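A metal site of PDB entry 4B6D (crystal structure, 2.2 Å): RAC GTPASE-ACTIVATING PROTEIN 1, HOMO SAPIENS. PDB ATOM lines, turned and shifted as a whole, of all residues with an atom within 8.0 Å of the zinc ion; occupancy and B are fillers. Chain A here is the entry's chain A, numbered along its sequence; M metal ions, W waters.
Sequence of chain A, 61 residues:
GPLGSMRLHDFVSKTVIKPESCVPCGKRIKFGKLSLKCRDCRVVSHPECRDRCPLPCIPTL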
ATOM      1  N   SER A  21      -1.044  -2.031 -11.808  1.00  0.00           N
ATOM      2  CA  SER A  21      -0.701  -1.297 -10.602  1.00  0.00           C
ATOM      3  C   SER A  21       0.115  -0.059 -10.954  1.00  0.00           C
ATOM      4  O   SER A  21       1.144  -0.150 -11.623  1.00  0.00           O
ATOM      5  CB  SER A  21       0.101  -2.185  -9.645  1.00  0.00           C
ATOM      6  OG  SER A  21       0.425  -1.488  -8.457  1.00  0.00           O
ATOM      7  N   CYS A  22      -0.353   1.103 -10.503  1.00  0.00           N
ATOM      8  CA  CYS A  22       0.338   2.357 -10.751  1.00  0.00           C
ATOM      9  C   CYS A  22       1.684   2.350 -10.028  1.00  0.00           C
ATOM     10  O   CYS A  22       1.749   2.079  -8.840  1.00  0.00           O
ATOM     11  CB  CYS A  22      -0.503   3.531 -10.266  1.00  0.00           C
ATOM     12  SG  CYS A  22       0.224   5.168 -10.523  1.00  0.00           S
ATOM     13  N   VAL A  23       2.750   2.618 -10.762  1.00  0.00           N
ATOM     14  CA  VAL A  23       4.095   2.596 -10.176  1.00  0.00           C
ATOM     15  C   VAL A  23       4.340   3.693  -9.120  1.00  0.00           C
ATOM     16  O   VAL A  23       4.859   3.389  -8.046  1.00  0.00           O
ATOM     17  CB  VAL A  23       5.216   2.582 -11.259  1.00  0.00           C
ATOM     18  CG1 VAL A  23       6.586   2.678 -10.615  1.00  0.00           C
ATOM     19  CG2 VAL A  23       5.097   1.345 -12.131  1.00  0.00           C
ATOM     20  N   PRO A  24       3.959   4.950  -9.408  1.00  0.00           N
ATOM     21  CA  PRO A  24       4.176   5.960  -8.360  1.00  0.00           C
ATOM     22  C   PRO A  24       3.336   5.777  -7.102  1.00  0.00           C
ATOM     23  O   PRO A  24       3.888   5.878  -5.997  1.00  0.00           O
ATOM     24  CB  PRO A  24       3.793   7.289  -9.035  1.00  0.00           C
ATOM     25  CG  PRO A  24       3.449   6.982 -10.430  1.00  0.00           C
ATOM     26  CD  PRO A  24       3.694   5.557 -10.726  1.00  0.00           C
ATOM     27  N   CYS A  25       2.045   5.523  -7.237  1.00  0.00           N
ATOM     28  CA  CYS A  25       1.157   5.497  -6.065  1.00  0.00           C
ATOM     29  C   CYS A  25       0.902   4.089  -5.529  1.00  0.00           C
ATOM     30  O   CYS A  25       0.394   3.927  -4.420  1.00  0.00           O
ATOM     31  CB  CYS A  25      -0.161   6.215  -6.354  1.00  0.00           C
ATOM     32  SG  CYS A  25      -1.379   5.289  -7.335  1.00  0.00           S
ATOM     33  N   GLY A  26       1.231   3.076  -6.313  1.00  0.00           N
ATOM     34  CA  GLY A  26       1.086   1.693  -5.878  1.00  0.00           C
ATOM     35  C   GLY A  26      -0.317   1.142  -5.992  1.00  0.00           C
ATOM     36  O   GLY A  26      -0.526  -0.059  -5.880  1.00  0.00           O
ATOM     37  N   LYS A  27      -1.293   2.022  -6.239  1.00  0.00           N
ATOM     38  CA  LYS A  27      -2.685   1.588  -6.321  1.00  0.00           C
ATOM     39  C   LYS A  27      -3.028   1.000  -7.685  1.00  0.00           C
ATOM     40  O   LYS A  27      -2.343   1.263  -8.672  1.00  0.00           O
ATOM     41  CB  LYS A  27      -3.629   2.746  -5.968  1.00  0.00           C
ATOM     42  CG  LYS A  27      -3.872   2.920  -4.487  1.00  0.00           C
ATOM     43  CD  LYS A  27      -4.927   3.979  -4.202  1.00  0.00           C
ATOM     44  CE  LYS A  27      -5.244   4.052  -2.713  1.00  0.00           C
ATOM     45  NZ  LYS A  27      -4.275   3.278  -1.900  1.00  0.00           N
ATOM     46  N   ARG A  28      -4.087   0.210  -7.719  1.00  0.00           N
ATOM     47  CA  ARG A  28      -4.519  -0.456  -8.943  1.00  0.00           C
ATOM     48  C   ARG A  28      -5.262   0.488  -9.890  1.00  0.00           C
ATOM     49  O   ARG A  28      -6.096   1.293  -9.471  1.00  0.00           O
ATOM     50  CB  ARG A  28      -5.389  -1.670  -8.622  1.00  0.00           C
ATOM     51  CG  ARG A  28      -6.818  -1.351  -8.205  1.00  0.00           C
ATOM     52  CD  ARG A  28      -7.623  -2.606  -7.919  1.00  0.00           C
ATOM     53  NE  ARG A  28      -7.664  -3.496  -9.078  1.00  0.00           N
ATOM     54  CZ  ARG A  28      -8.050  -4.772  -9.032  1.00  0.00           C
ATOM     55  NH1 ARG A  28      -8.432  -5.318  -7.880  1.00  0.00           N
ATOM     56  NH2 ARG A  28      -8.069  -5.502 -10.133  1.00  0.00           N
ATOM     57  N   ILE A  29      -4.908   0.412 -11.170  1.00  0.00           N
ATOM     58  CA  ILE A  29      -5.626   1.170 -12.189  1.00  0.00           C
ATOM     59  C   ILE A  29      -6.754   0.289 -12.717  1.00  0.00           C
ATOM     60  O   ILE A  29      -6.523  -0.723 -13.377  1.00  0.00           O
ATOM     61  CB  ILE A  29      -4.713   1.589 -13.356  1.00  0.00           C
ATOM     62  CG1 ILE A  29      -3.370   2.086 -12.816  1.00  0.00           C
ATOM     63  CG2 ILE A  29      -5.385   2.665 -14.187  1.00  0.00           C
ATOM     64  CD1 ILE A  29      -2.379   2.419 -13.905  1.00  0.00           C
ATOM     65  N   VAL A  44       4.064   1.911 -15.798  1.00  0.00           N
ATOM     66  CA  VAL A  44       2.665   2.208 -16.058  1.00  0.00           C
ATOM     67  C   VAL A  44       2.127   3.031 -14.880  1.00  0.00           C
ATOM     68  O   VAL A  44       2.542   2.809 -13.742  1.00  0.00           O
ATOM     69  CB  VAL A  44       1.831   0.923 -16.245  1.00  0.00           C
ATOM     70  CG1 VAL A  44       1.956   0.018 -15.032  1.00  0.00           C
ATOM     71  CG2 VAL A  44       0.372   1.248 -16.531  1.00  0.00           C
ATOM     72  N   SER A  45       1.252   3.980 -15.148  1.00  0.00           N
ATOM     73  CA  SER A  45       0.755   4.867 -14.096  1.00  0.00           C
ATOM     74  C   SER A  45      -0.603   5.482 -14.392  1.00  0.00           C
ATOM     75  O   SER A  45      -1.072   5.446 -15.531  1.00  0.00           O
ATOM     76  CB  SER A  45       1.780   5.981 -13.841  1.00  0.00           C
ATOM     77  OG  SER A  45       1.258   6.982 -12.989  1.00  0.00           O
ATOM     78  N   HIS A  46      -1.217   6.052 -13.368  1.00  0.00           N
ATOM     79  CA  HIS A  46      -2.410   6.871 -13.562  1.00  0.00           C
ATOM     80  C   HIS A  46      -1.977   8.103 -14.331  1.00  0.00           C
ATOM     81  O   HIS A  46      -0.830   8.542 -14.206  1.00  0.00           O
ATOM     82  CB  HIS A  46      -3.015   7.306 -12.220  1.00  0.00           C
ATOM     83  CG  HIS A  46      -3.586   6.193 -11.398  1.00  0.00           C
ATOM     84  ND1 HIS A  46      -2.957   5.698 -10.279  1.00  0.00           N
ATOM     85  CD2 HIS A  46      -4.732   5.482 -11.543  1.00  0.00           C
ATOM     86  CE1 HIS A  46      -3.695   4.724  -9.762  1.00  0.00           C
ATOM     87  NE2 HIS A  46      -4.777   4.576 -10.513  1.00  0.00           N
ATOM     88  N   PRO A  47      -2.889   8.676 -15.137  1.00  0.00           N
ATOM     89  CA  PRO A  47      -2.612   9.930 -15.829  1.00  0.00           C
ATOM     90  C   PRO A  47      -2.222  11.041 -14.853  1.00  0.00           C
ATOM     91  O   PRO A  47      -1.377  11.880 -15.175  1.00  0.00           O
ATOM     92  CB  PRO A  47      -3.944  10.261 -16.496  1.00  0.00           C
ATOM     93  CG  PRO A  47      -4.580   8.923 -16.717  1.00  0.00           C
ATOM     94  CD  PRO A  47      -4.190   8.103 -15.518  1.00  0.00           C
ATOM     95  N   GLU A  48      -2.834  11.030 -13.669  1.00  0.00           N
ATOM     96  CA  GLU A  48      -2.591  12.058 -12.656  1.00  0.00           C
ATOM     97  C   GLU A  48      -1.337  11.817 -11.806  1.00  0.00           C
ATOM     98  O   GLU A  48      -0.942  12.669 -11.017  1.00  0.00           O
ATOM     99  CB  GLU A  48      -3.821  12.206 -11.754  1.00  0.00           C
ATOM    100  CG  GLU A  48      -4.203  10.932 -11.017  1.00  0.00           C
ATOM    101  CD  GLU A  48      -5.141  10.046 -11.808  1.00  0.00           C
ATOM    102  OE1 GLU A  48      -5.287  10.272 -13.033  1.00  0.00           O
ATOM    103  OE2 GLU A  48      -5.728   9.122 -11.215  1.00  0.00           O
ATOM    104  N   CYS A  49      -0.709  10.656 -11.980  1.00  0.00           N
ATOM    105  CA  CYS A  49       0.489  10.320 -11.214  1.00  0.00           C
ATOM    106  C   CYS A  49       1.717  10.349 -12.122  1.00  0.00           C
ATOM    107  O   CYS A  49       2.810   9.955 -11.712  1.00  0.00           O
ATOM    108  CB  CYS A  49       0.352   8.939 -10.569  1.00  0.00           C
ATOM    109  SG  CYS A  49      -1.034   8.748  -9.420  1.00  0.00           S
ATOM    110  N   ARG A  50       1.520  10.805 -13.354  1.00  0.00           N
ATOM    111  CA  ARG A  50       2.556  10.836 -14.391  1.00  0.00           C
ATOM    112  C   ARG A  50       3.881  11.519 -14.036  1.00  0.00           C
ATOM    113  O   ARG A  50       4.950  11.017 -14.377  1.00  0.00           O
ATOM    114  CB  ARG A  50       1.973  11.475 -15.657  1.00  0.00           C
ATOM    115  CG  ARG A  50       2.959  11.567 -16.807  1.00  0.00           C
ATOM    116  CD  ARG A  50       2.330  12.302 -17.986  1.00  0.00           C
ATOM    117  NE  ARG A  50       1.499  13.416 -17.554  1.00  0.00           N
ATOM    118  CZ  ARG A  50       1.877  14.686 -17.603  1.00  0.00           C
ATOM    119  NH1 ARG A  50       3.084  15.003 -18.063  1.00  0.00           N
ATOM    120  NH2 ARG A  50       1.055  15.645 -17.190  1.00  0.00           N
ATOM    121  N   ARG A  52       5.324  11.891 -11.249  1.00  0.00           N
ATOM    122  CA  ARG A  52       6.000  11.248 -10.123  1.00  0.00           C
ATOM    123  C   ARG A  52       6.641   9.911 -10.458  1.00  0.00           C
ATOM    124  O   ARG A  52       7.161   9.226  -9.579  1.00  0.00           O
ATOM    125  CB  ARG A  52       5.016  11.097  -8.976  1.00  0.00           C
ATOM    126  CG  ARG A  52       4.607  12.408  -8.342  1.00  0.00           C
ATOM    127  CD  ARG A  52       4.062  12.166  -6.961  1.00  0.00           C
ATOM    128  NE  ARG A  52       2.657  11.809  -7.047  1.00  0.00           N
ATOM    129  CZ  ARG A  52       2.184  10.568  -6.965  1.00  0.00           C
ATOM    130  NH1 ARG A  52       3.022   9.553  -6.784  1.00  0.00           N
ATOM    131  NH2 ARG A  52       0.883  10.340  -7.053  1.00  0.00           N
ATOM    132  N   CYS A  53       6.593   9.529 -11.733  1.00  0.00           N
ATOM    133  CA  CYS A  53       7.197   8.279 -12.188  1.00  0.00           C
ATOM    134  C   CYS A  53       8.712   8.361 -12.073  1.00  0.00           C
ATOM    135  O   CYS A  53       9.317   9.346 -12.488  1.00  0.00           O
ATOM    136  CB  CYS A  53       6.787   7.955 -13.610  1.00  0.00           C
ATOM    137  SG  CYS A  53       5.067   7.446 -13.796  1.00  0.00           S
HETATM  138 ZN    ZN M   1      -1.306   6.439  -9.312  1.00  0.00          ZN
HETATM  139  O   HOH W   1      -3.545   7.602  -7.063  1.00  0.00           O
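The side-chain sulfur (SG) of Cys 22 sits close to the side-chain hydroxyl (OG) of Ser 45. N of Cys 22 lies within hydrogen-bond range of O of Lys 27 (2.7 Å). The backbone NH (N) of Lys 27 lies close to the side-chain sulfur (SG) of Cys 25 (3.4 Å). NH2 of Arg 52 sits close to SG of Cys 49.
Of the 18 residues printed, 4 come within 4 Å of the zinc ion.
The zinc ion is bound by a ring nitrogen (ND1) of His 46 (2.1 Å), the side-chain sulfur (SG) of Cys 25 (2.3 Å), the side-chain sulfur (SG) of Cys 49 (2.3 Å) and the side-chain sulfur (SG) of Cys 22 (2.3 Å). The zinc ion has four donor atoms within binding distance.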
